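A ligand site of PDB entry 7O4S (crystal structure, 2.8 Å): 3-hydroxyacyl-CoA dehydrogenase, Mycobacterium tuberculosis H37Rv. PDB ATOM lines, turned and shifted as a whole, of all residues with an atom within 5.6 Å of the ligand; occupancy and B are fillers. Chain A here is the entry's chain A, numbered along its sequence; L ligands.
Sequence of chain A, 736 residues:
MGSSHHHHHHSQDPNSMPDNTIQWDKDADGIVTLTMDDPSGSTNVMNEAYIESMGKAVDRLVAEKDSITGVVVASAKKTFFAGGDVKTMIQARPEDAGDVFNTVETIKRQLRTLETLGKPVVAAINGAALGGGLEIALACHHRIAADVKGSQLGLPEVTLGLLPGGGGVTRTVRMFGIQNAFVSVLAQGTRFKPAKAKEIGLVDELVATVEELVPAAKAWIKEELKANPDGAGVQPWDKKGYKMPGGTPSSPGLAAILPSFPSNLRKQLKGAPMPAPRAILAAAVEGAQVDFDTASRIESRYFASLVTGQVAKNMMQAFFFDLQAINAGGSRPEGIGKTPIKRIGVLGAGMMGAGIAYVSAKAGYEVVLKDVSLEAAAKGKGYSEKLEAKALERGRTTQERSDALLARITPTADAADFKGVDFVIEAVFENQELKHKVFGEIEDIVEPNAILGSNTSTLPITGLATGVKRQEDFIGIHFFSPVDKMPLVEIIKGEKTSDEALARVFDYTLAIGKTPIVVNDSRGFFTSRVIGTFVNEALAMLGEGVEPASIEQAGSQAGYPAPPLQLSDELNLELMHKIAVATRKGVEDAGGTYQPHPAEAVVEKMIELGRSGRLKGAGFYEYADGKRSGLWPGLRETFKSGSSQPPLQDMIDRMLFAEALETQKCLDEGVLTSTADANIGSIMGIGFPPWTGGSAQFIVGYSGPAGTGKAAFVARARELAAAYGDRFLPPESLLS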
ATOM      1  N   SER A  42     -16.582  -7.684   8.398  1.00  0.00           N
ATOM      2  CA  SER A  42     -16.052  -6.376   8.037  1.00  0.00           C
ATOM      3  C   SER A  42     -15.364  -6.377   6.675  1.00  0.00           C
ATOM      4  O   SER A  42     -14.765  -5.371   6.295  1.00  0.00           O
ATOM      5  CB  SER A  42     -15.077  -5.884   9.111  1.00  0.00           C
ATOM      6  OG  SER A  42     -14.051  -6.829   9.333  1.00  0.00           O
ATOM      7  N   THR A  43     -15.430  -7.486   5.945  1.00  0.00           N
ATOM      8  CA  THR A  43     -14.780  -7.577   4.637  1.00  0.00           C
ATOM      9  C   THR A  43     -15.601  -8.493   3.746  1.00  0.00           C
ATOM     10  O   THR A  43     -16.372  -9.329   4.216  1.00  0.00           O
ATOM     11  CB  THR A  43     -13.335  -8.082   4.757  1.00  0.00           C
ATOM     12  OG1 THR A  43     -12.666  -7.921   3.506  1.00  0.00           O
ATOM     13  CG2 THR A  43     -13.315  -9.548   5.166  1.00  0.00           C
ATOM     14  N   VAL A  45     -15.725 -11.511   1.218  1.00  0.00           N
ATOM     15  CA  VAL A  45     -14.985 -12.720   0.896  1.00  0.00           C
ATOM     16  C   VAL A  45     -15.878 -13.641   0.054  1.00  0.00           C
ATOM     17  O   VAL A  45     -17.091 -13.445  -0.044  1.00  0.00           O
ATOM     18  CB  VAL A  45     -14.476 -13.463   2.146  1.00  0.00           C
ATOM     19  CG1 VAL A  45     -13.481 -12.601   2.905  1.00  0.00           C
ATOM     20  CG2 VAL A  45     -15.643 -13.863   3.030  1.00  0.00           C
ATOM     21  N   LYS A  78     -14.289  -0.754   3.848  1.00  0.00           N
ATOM     22  CA  LYS A  78     -12.976  -0.137   3.713  1.00  0.00           C
ATOM     23  C   LYS A  78     -12.197  -0.746   2.561  1.00  0.00           C
ATOM     24  O   LYS A  78     -11.498  -0.046   1.830  1.00  0.00           O
ATOM     25  CB  LYS A  78     -12.179  -0.277   5.010  1.00  0.00           C
ATOM     26  CG  LYS A  78     -12.834   0.368   6.227  1.00  0.00           C
ATOM     27  CD  LYS A  78     -11.953   0.215   7.455  1.00  0.00           C
ATOM     28  CE  LYS A  78     -12.615   0.776   8.696  1.00  0.00           C
ATOM     29  NZ  LYS A  78     -11.745   0.633   9.894  1.00  0.00           N
ATOM     30  N   THR A  79     -12.325  -2.064   2.377  1.00  0.00           N
ATOM     31  CA  THR A  79     -11.633  -2.784   1.316  1.00  0.00           C
ATOM     32  C   THR A  79     -12.626  -3.155   0.210  1.00  0.00           C
ATOM     33  O   THR A  79     -13.823  -3.315   0.459  1.00  0.00           O
ATOM     34  CB  THR A  79     -10.970  -4.043   1.851  1.00  0.00           C
ATOM     35  OG1 THR A  79     -11.944  -4.855   2.530  1.00  0.00           O
ATOM     36  CG2 THR A  79      -9.850  -3.682   2.818  1.00  0.00           C
ATOM     37  N   ALA A  82     -11.645  -9.064  -0.305  1.00  0.00           N
ATOM     38  CA  ALA A  82     -10.506  -9.713   0.321  1.00  0.00           C
ATOM     39  C   ALA A  82     -10.187 -11.095  -0.251  1.00  0.00           C
ATOM     40  O   ALA A  82      -9.192 -11.692   0.155  1.00  0.00           O
ATOM     41  CB  ALA A  82     -10.726  -9.809   1.824  1.00  0.00           C
ATOM     42  N   GLY A  83     -11.019 -11.627  -1.145  1.00  0.00           N
ATOM     43  CA  GLY A  83     -10.686 -12.902  -1.760  1.00  0.00           C
ATOM     44  C   GLY A  83     -11.381 -14.110  -1.174  1.00  0.00           C
ATOM     45  O   GLY A  83     -12.451 -13.988  -0.573  1.00  0.00           O
ATOM     46  N   GLY A  84     -10.782 -15.292  -1.326  1.00  0.00           N
ATOM     47  CA  GLY A  84     -11.432 -16.503  -0.881  1.00  0.00           C
ATOM     48  C   GLY A  84     -11.484 -16.633   0.633  1.00  0.00           C
ATOM     49  O   GLY A  84     -10.697 -16.048   1.369  1.00  0.00           O
ATOM     50  N   ASP A  85     -12.457 -17.410   1.093  1.00  0.00           N
ATOM     51  CA  ASP A  85     -12.664 -17.641   2.527  1.00  0.00           C
ATOM     52  C   ASP A  85     -11.624 -18.652   3.006  1.00  0.00           C
ATOM     53  O   ASP A  85     -11.759 -19.858   2.800  1.00  0.00           O
ATOM     54  CB  ASP A  85     -14.080 -18.142   2.789  1.00  0.00           C
ATOM     55  CG  ASP A  85     -14.503 -17.972   4.227  1.00  0.00           C
ATOM     56  OD1 ASP A  85     -13.613 -17.927   5.108  1.00  0.00           O
ATOM     57  OD2 ASP A  85     -15.720 -17.881   4.483  1.00  0.00           O
ATOM     58  N   VAL A  86     -10.558 -18.146   3.632  1.00  0.00           N
ATOM     59  CA  VAL A  86      -9.491 -19.011   4.121  1.00  0.00           C
ATOM     60  C   VAL A  86     -10.024 -19.980   5.167  1.00  0.00           C
ATOM     61  O   VAL A  86      -9.514 -21.105   5.308  1.00  0.00           O
ATOM     62  CB  VAL A  86      -8.325 -18.169   4.671  1.00  0.00           C
ATOM     63  CG1 VAL A  86      -7.151 -19.051   5.071  1.00  0.00           C
ATOM     64  CG2 VAL A  86      -7.893 -17.136   3.638  1.00  0.00           C
ATOM     65  N   LYS A  87     -11.044 -19.566   5.920  1.00  0.00           N
ATOM     66  CA  LYS A  87     -11.621 -20.448   6.932  1.00  0.00           C
ATOM     67  C   LYS A  87     -12.290 -21.661   6.304  1.00  0.00           C
ATOM     68  O   LYS A  87     -12.372 -22.722   6.940  1.00  0.00           O
ATOM     69  CB  LYS A  87     -12.602 -19.659   7.792  1.00  0.00           C
ATOM     70  CG  LYS A  87     -12.015 -18.362   8.334  1.00  0.00           C
ATOM     71  CD  LYS A  87     -13.017 -17.562   9.134  1.00  0.00           C
ATOM     72  CE  LYS A  87     -12.400 -16.245   9.607  1.00  0.00           C
ATOM     73  NZ  LYS A  87     -13.332 -15.447  10.449  1.00  0.00           N
ATOM     74  N   MET A  89     -11.382 -22.751   2.935  1.00  0.00           N
ATOM     75  CA  MET A  89     -10.418 -23.430   2.072  1.00  0.00           C
ATOM     76  C   MET A  89      -9.466 -24.324   2.859  1.00  0.00           C
ATOM     77  O   MET A  89      -8.995 -25.339   2.335  1.00  0.00           O
ATOM     78  CB  MET A  89      -9.626 -22.405   1.255  1.00  0.00           C
ATOM     79  CG  MET A  89     -10.480 -21.586   0.305  1.00  0.00           C
ATOM     80  SD  MET A  89      -9.505 -20.523  -0.777  1.00  0.00           S
ATOM     81  CE  MET A  89      -8.791 -19.369   0.389  1.00  0.00           C
ATOM     82  N   ALA A 128      -8.547  -2.245  -0.488  1.00  0.00           N
ATOM     83  CA  ALA A 128      -7.745  -3.387  -0.895  1.00  0.00           C
ATOM     84  C   ALA A 128      -8.577  -4.371  -1.709  1.00  0.00           C
ATOM     85  O   ALA A 128      -9.737  -4.652  -1.388  1.00  0.00           O
ATOM     86  CB  ALA A 128      -7.150  -4.093   0.320  1.00  0.00           C
ATOM     87  N   LEU A 130      -7.542  -8.017  -2.988  1.00  0.00           N
ATOM     88  CA  LEU A 130      -6.482  -9.017  -2.920  1.00  0.00           C
ATOM     89  C   LEU A 130      -7.053 -10.399  -3.216  1.00  0.00           C
ATOM     90  O   LEU A 130      -8.080 -10.796  -2.660  1.00  0.00           O
ATOM     91  CB  LEU A 130      -5.835  -9.005  -1.534  1.00  0.00           C
ATOM     92  CG  LEU A 130      -5.175  -7.685  -1.160  1.00  0.00           C
ATOM     93  CD1 LEU A 130      -4.465  -7.801   0.178  1.00  0.00           C
ATOM     94  CD2 LEU A 130      -4.201  -7.252  -2.236  1.00  0.00           C
ATOM     95  N   GLY A 131      -6.364 -11.132  -4.098  1.00  0.00           N
ATOM     96  CA  GLY A 131      -6.767 -12.474  -4.449  1.00  0.00           C
ATOM     97  C   GLY A 131      -8.045 -12.515  -5.246  1.00  0.00           C
ATOM     98  O   GLY A 131      -8.126 -11.938  -6.330  1.00  0.00           O
ATOM     99  N   GLY A 132      -9.068 -13.184  -4.709  1.00  0.00           N
ATOM    100  CA  GLY A 132     -10.360 -13.217  -5.375  1.00  0.00           C
ATOM    101  C   GLY A 132     -10.930 -11.831  -5.609  1.00  0.00           C
ATOM    102  O   GLY A 132     -11.715 -11.632  -6.541  1.00  0.00           O
ATOM    103  N   GLU A 135      -9.397 -10.723  -8.744  1.00  0.00           N
ATOM    104  CA  GLU A 135      -9.938 -11.583  -9.806  1.00  0.00           C
ATOM    105  C   GLU A 135     -11.310 -11.094 -10.266  1.00  0.00           C
ATOM    106  O   GLU A 135     -11.648 -11.242 -11.446  1.00  0.00           O
ATOM    107  CB  GLU A 135     -10.015 -13.029  -9.316  1.00  0.00           C
ATOM    108  CG  GLU A 135      -8.659 -13.640  -9.035  1.00  0.00           C
ATOM    109  CD  GLU A 135      -8.758 -15.071  -8.535  1.00  0.00           C
ATOM    110  OE1 GLU A 135      -9.535 -15.320  -7.593  1.00  0.00           O
ATOM    111  OE2 GLU A 135      -8.076 -15.937  -9.105  1.00  0.00           O
ATOM    112  N   GLN A 152      -4.243  -1.917  -1.202  1.00  0.00           N
ATOM    113  CA  GLN A 152      -3.335  -2.854  -1.834  1.00  0.00           C
ATOM    114  C   GLN A 152      -4.070  -3.643  -2.904  1.00  0.00           C
ATOM    115  O   GLN A 152      -5.269  -3.894  -2.802  1.00  0.00           O
ATOM    116  CB  GLN A 152      -2.722  -3.828  -0.818  1.00  0.00           C
ATOM    117  CG  GLN A 152      -1.747  -3.197   0.155  1.00  0.00           C
ATOM    118  CD  GLN A 152      -1.213  -4.184   1.168  1.00  0.00           C
ATOM    119  OE1 GLN A 152      -1.944  -5.074   1.625  1.00  0.00           O
ATOM    120  NE2 GLN A 152       0.053  -4.053   1.520  1.00  0.00           N
ATOM    121  N   PRO A 156      -2.118 -12.617  -3.947  1.00  0.00           N
ATOM    122  CA  PRO A 156      -1.154 -13.233  -3.041  1.00  0.00           C
ATOM    123  C   PRO A 156      -1.503 -14.664  -2.666  1.00  0.00           C
ATOM    124  O   PRO A 156      -1.189 -15.114  -1.559  1.00  0.00           O
ATOM    125  CB  PRO A 156      -1.204 -12.318  -1.815  1.00  0.00           C
ATOM    126  CG  PRO A 156      -2.625 -11.859  -1.788  1.00  0.00           C
ATOM    127  CD  PRO A 156      -3.094 -11.777  -3.234  1.00  0.00           C
ATOM    128  N   GLU A 157      -2.150 -15.399  -3.570  1.00  0.00           N
ATOM    129  CA  GLU A 157      -2.559 -16.766  -3.252  1.00  0.00           C
ATOM    130  C   GLU A 157      -1.362 -17.692  -3.055  1.00  0.00           C
ATOM    131  O   GLU A 157      -1.446 -18.641  -2.270  1.00  0.00           O
ATOM    132  CB  GLU A 157      -3.472 -17.317  -4.359  1.00  0.00           C
ATOM    133  CG  GLU A 157      -4.922 -16.888  -4.254  1.00  0.00           C
ATOM    134  CD  GLU A 157      -5.235 -15.664  -5.096  1.00  0.00           C
ATOM    135  OE1 GLU A 157      -4.329 -14.835  -5.283  1.00  0.00           O
ATOM    136  OE2 GLU A 157      -6.384 -15.555  -5.570  1.00  0.00           O
ATOM    137  N   THR A 159       1.393 -17.131  -1.584  1.00  0.00           N
ATOM    138  CA  THR A 159       1.934 -17.012  -0.233  1.00  0.00           C
ATOM    139  C   THR A 159       1.181 -17.871   0.766  1.00  0.00           C
ATOM    140  O   THR A 159       1.725 -18.169   1.838  1.00  0.00           O
ATOM    141  CB  THR A 159       1.910 -15.553   0.209  1.00  0.00           C
ATOM    142  OG1 THR A 159       0.566 -15.057   0.170  1.00  0.00           O
ATOM    143  CG2 THR A 159       2.783 -14.701  -0.709  1.00  0.00           C
ATOM    144  N   LEU A 160      -0.056 -18.253   0.458  1.00  0.00           N
ATOM    145  CA  LEU A 160      -0.823 -19.174   1.282  1.00  0.00           C
ATOM    146  C   LEU A 160      -0.813 -20.597   0.732  1.00  0.00           C
ATOM    147  O   LEU A 160      -1.574 -21.433   1.212  1.00  0.00           O
ATOM    148  CB  LEU A 160      -2.264 -18.675   1.413  1.00  0.00           C
ATOM    149  CG  LEU A 160      -2.444 -17.284   2.038  1.00  0.00           C
ATOM    150  CD1 LEU A 160      -3.907 -16.868   1.991  1.00  0.00           C
ATOM    151  CD2 LEU A 160      -1.929 -17.276   3.471  1.00  0.00           C
ATOM    152  N   LEU A 162      -1.618 -21.462  -2.410  1.00  0.00           N
ATOM    153  CA  LEU A 162      -2.681 -21.609  -3.391  1.00  0.00           C
ATOM    154  C   LEU A 162      -2.251 -20.963  -4.712  1.00  0.00           C
ATOM    155  O   LEU A 162      -1.073 -20.627  -4.909  1.00  0.00           O
ATOM    156  CB  LEU A 162      -3.982 -20.981  -2.869  1.00  0.00           C
ATOM    157  CG  LEU A 162      -4.390 -21.345  -1.447  1.00  0.00           C
ATOM    158  CD1 LEU A 162      -5.604 -20.546  -1.012  1.00  0.00           C
ATOM    159  CD2 LEU A 162      -4.661 -22.838  -1.336  1.00  0.00           C
ATOM    160  N   ARG A 191       1.972  -7.594  -3.275  1.00  0.00           N
ATOM    161  CA  ARG A 191       0.909  -6.608  -3.135  1.00  0.00           C
ATOM    162  C   ARG A 191       1.415  -5.257  -3.593  1.00  0.00           C
ATOM    163  O   ARG A 191       2.523  -4.838  -3.234  1.00  0.00           O
ATOM    164  CB  ARG A 191       0.431  -6.539  -1.684  1.00  0.00           C
ATOM    165  CG  ARG A 191       0.072  -7.886  -1.083  1.00  0.00           C
ATOM    166  CD  ARG A 191      -0.550  -7.724   0.301  1.00  0.00           C
ATOM    167  NE  ARG A 191      -0.969  -9.007   0.856  1.00  0.00           N
ATOM    168  CZ  ARG A 191      -1.709  -9.139   1.957  1.00  0.00           C
ATOM    169  NH1 ARG A 191      -2.044 -10.349   2.388  1.00  0.00           N
ATOM    170  NH2 ARG A 191      -2.113  -8.061   2.617  1.00  0.00           N
ATOM    171  N   PHE A 320      -1.699 -16.916   7.591  1.00  0.00           N
ATOM    172  CA  PHE A 320      -2.971 -16.207   7.728  1.00  0.00           C
ATOM    173  C   PHE A 320      -3.433 -16.236   9.172  1.00  0.00           C
ATOM    174  O   PHE A 320      -3.538 -15.191   9.825  1.00  0.00           O
ATOM    175  CB  PHE A 320      -4.048 -16.787   6.817  1.00  0.00           C
ATOM    176  CG  PHE A 320      -5.362 -16.062   6.905  1.00  0.00           C
ATOM    177  CD1 PHE A 320      -5.579 -14.893   6.201  1.00  0.00           C
ATOM    178  CD2 PHE A 320      -6.389 -16.556   7.705  1.00  0.00           C
ATOM    179  CE1 PHE A 320      -6.784 -14.220   6.287  1.00  0.00           C
ATOM    180  CE2 PHE A 320      -7.602 -15.895   7.790  1.00  0.00           C
ATOM    181  CZ  PHE A 320      -7.800 -14.723   7.086  1.00  0.00           C
ATOM    182  N   GLN A 324      -2.174 -13.532  12.009  1.00  0.00           N
ATOM    183  CA  GLN A 324      -3.178 -12.589  12.469  1.00  0.00           C
ATOM    184  C   GLN A 324      -3.362 -12.659  13.984  1.00  0.00           C
ATOM    185  O   GLN A 324      -3.584 -11.642  14.633  1.00  0.00           O
ATOM    186  CB  GLN A 324      -4.508 -12.828  11.767  1.00  0.00           C
ATOM    187  CG  GLN A 324      -4.584 -12.229  10.374  1.00  0.00           C
ATOM    188  CD  GLN A 324      -5.994 -12.247   9.807  1.00  0.00           C
ATOM    189  OE1 GLN A 324      -6.934 -12.697  10.471  1.00  0.00           O
ATOM    190  NE2 GLN A 324      -6.148 -11.764   8.585  1.00  0.00           N
HETATM  191  N1  LIG L   1     -10.836 -15.007   4.297  1.00  0.00           N
HETATM  192  C1  LIG L   1     -11.497 -15.009   5.458  1.00  0.00           C
HETATM  193  N2  LIG L   1     -11.585 -14.049   6.376  1.00  0.00           N
HETATM  194  C2  LIG L   1     -10.887 -12.967   6.002  1.00  0.00           C
HETATM  195  C3  LIG L   1     -10.159 -12.812   4.843  1.00  0.00           C
HETATM  196  C4  LIG L   1     -10.142 -13.897   3.945  1.00  0.00           C
HETATM  197  N3  LIG L   1      -9.481 -13.895   2.784  1.00  0.00           N
HETATM  198  N4  LIG L   1      -9.569 -11.556   4.800  1.00  0.00           N
HETATM  199  C5  LIG L   1      -9.946 -10.982   5.927  1.00  0.00           C
HETATM  200  N5  LIG L   1     -10.740 -11.791   6.688  1.00  0.00           N
HETATM  201  C6  LIG L   1     -11.334 -11.477   7.993  1.00  0.00           C
HETATM  202  C7  LIG L   1     -10.481 -11.826   9.197  1.00  0.00           C
HETATM  203  O1  LIG L   1     -10.421 -13.206   9.483  1.00  0.00           O
HETATM  204  C8  LIG L   1     -11.162 -10.993  10.276  1.00  0.00           C
HETATM  205  O2  LIG L   1     -12.332 -11.680  10.729  1.00  0.00           O
HETATM  206  P1  LIG L   1     -12.621 -11.353  12.281  1.00  0.00           P
HETATM  207  O3  LIG L   1     -11.620 -12.179  13.083  1.00  0.00           O
HETATM  208  O4  LIG L   1     -12.419  -9.863  12.489  1.00  0.00           O
HETATM  209  O5  LIG L   1     -14.050 -11.776  12.557  1.00  0.00           O
HETATM  210  C9  LIG L   1     -11.594  -9.742   9.504  1.00  0.00           C
HETATM  211  O6  LIG L   1     -11.508 -10.091   8.097  1.00  0.00           O
HETATM  212  C10 LIG L   1     -10.775  -8.510   9.754  1.00  0.00           C
HETATM  213  O7  LIG L   1      -9.406  -8.758   9.339  1.00  0.00           O
HETATM  214  P2  LIG L   1      -8.285  -7.654   9.666  1.00  0.00           P
HETATM  215  O8  LIG L   1      -6.970  -8.116   9.136  1.00  0.00           O
HETATM  216  O9  LIG L   1      -8.376  -7.278  11.105  1.00  0.00           O
HETATM  217  O10 LIG L   1      -8.792  -6.418   8.781  1.00  0.00           O
HETATM  218  P3  LIG L   1      -8.007  -5.499   7.726  1.00  0.00           P
HETATM  219  O11 LIG L   1      -8.924  -4.427   7.224  1.00  0.00           O
HETATM  220  O12 LIG L   1      -6.689  -5.100   8.288  1.00  0.00           O
HETATM  221  O13 LIG L   1      -7.763  -6.559   6.544  1.00  0.00           O
HETATM  222  C11 LIG L   1      -6.928  -7.347   4.418  1.00  0.00           C
HETATM  223  C12 LIG L   1      -7.036  -6.148   5.362  1.00  0.00           C
HETATM  224  C13 LIG L   1      -8.329  -7.757   3.964  1.00  0.00           C
HETATM  225  C14 LIG L   1      -6.096  -6.948   3.197  1.00  0.00           C
HETATM  226  C15 LIG L   1      -6.254  -8.525   5.139  1.00  0.00           C
HETATM  227  O14 LIG L   1      -7.192  -9.151   6.012  1.00  0.00           O
HETATM  228  C16 LIG L   1      -5.626  -9.559   4.216  1.00  0.00           C
HETATM  229  O15 LIG L   1      -4.415  -9.565   4.046  1.00  0.00           O
HETATM  230  N6  LIG L   1      -6.430 -10.454   3.658  1.00  0.00           N
HETATM  231  C17 LIG L   1      -5.927 -11.636   2.963  1.00  0.00           C
HETATM  232  C18 LIG L   1      -6.332 -11.695   1.508  1.00  0.00           C
HETATM  233  C19 LIG L   1      -5.633 -12.833   0.779  1.00  0.00           C
HETATM  234  O16 LIG L   1      -4.408 -12.885   0.737  1.00  0.00           O
HETATM  235  N7  LIG L   1      -6.410 -13.762   0.200  1.00  0.00           N
HETATM  236  C20 LIG L   1      -5.858 -14.939  -0.454  1.00  0.00           C
HETATM  237  C21 LIG L   1      -6.938 -15.893  -0.941  1.00  0.00           C
HETATM  238  S1  LIG L   1      -7.897 -15.284  -2.349  1.00  0.00           S
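A sulfur (S1) of the ligand lies close to the side-chain carboxylate (OE2) of Glu 157 (3.6 Å).
The backbone carbonyl oxygen (O) of Gly 84 sits at hydrogen-bond distance from a nitrogen (N3) of the ligand, at 2.8 Å.
NH1 of Arg 191 is in hydrogen-bond range of O15 of the ligand (3.0 Å).
N of Gly 84 lies close to S1 of the ligand, 3.1 Å away.
The backbone carbonyl oxygen (O) of Ala 82 lies close to a nitrogen (N3) of the ligand, 3.4 Å away.
N of Val 86 is in hydrogen-bond range of N1 of the ligand.
A sulfur (S1) of the ligand lies close to the backbone NH (N) of Gly 132 (3.4 Å).
The backbone carbonyl oxygen of Leu 130 lies within hydrogen-bond range of the backbone NH of Gly 83, at 3.4 Å.
O of Pro 156 lies within hydrogen-bond range of OG1 of Thr 159 (2.5 Å).
The guanidinium group (NH2) of Arg 191 is in hydrogen-bond range of the side-chain amide oxygen (OE1) of Gln 152 (3.2 Å).
OG1 of Thr 79 lies within hydrogen-bond range of OG1 of Thr 43 (3.3 Å).
OD1 of Asp 85 sits close to N of Lys 87 (3.2 Å).
The backbone NH (N) of Leu 162 is in hydrogen-bond range of the backbone carbonyl oxygen (O) of Glu 157 (2.8 Å).
Ser 42 touches the ligand (OG to C10, 3.7 Å).
Thr 43 touches the ligand (CG2 to O6, 3.5 Å).
CG1 of Val 45 touches C4 of the ligand (3.7 Å).
CA of Gly 83 touches S1 of the ligand, at 3.7 Å.
Asp 85 touches the ligand.
CE of Lys 87 touches O1 of the ligand, at 3.6 Å.
CD1 of Leu 130 touches C14 of the ligand, 3.5 Å away.
CA of Gly 131 touches S1 of the ligand, at 3.7 Å.
Pro 156 touches the ligand.
CD1 of Leu 160 touches C20 of the ligand (3.7 Å).
CZ of Phe 320 touches C2 of the ligand, at 3.7 Å.
Gln 324 touches the ligand (OE1 to O1, 3.7 Å).
Hydrophobic or aromatic side chains within 4 Å of the ligand: Val 45, Ala 82, Val 86, Leu 130, Pro 156, Leu 160 and Phe 320.
Within 4 Å of the ligand: Ser 42, Thr 43, Val 45, Ala 82, Gly 83, Gly 84, Asp 85, Val 86, Lys 87, Leu 130, Gly 131, Gly 132, Pro 156, Glu 157, Leu 160, Arg 191, Phe 320 and Gln 324.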
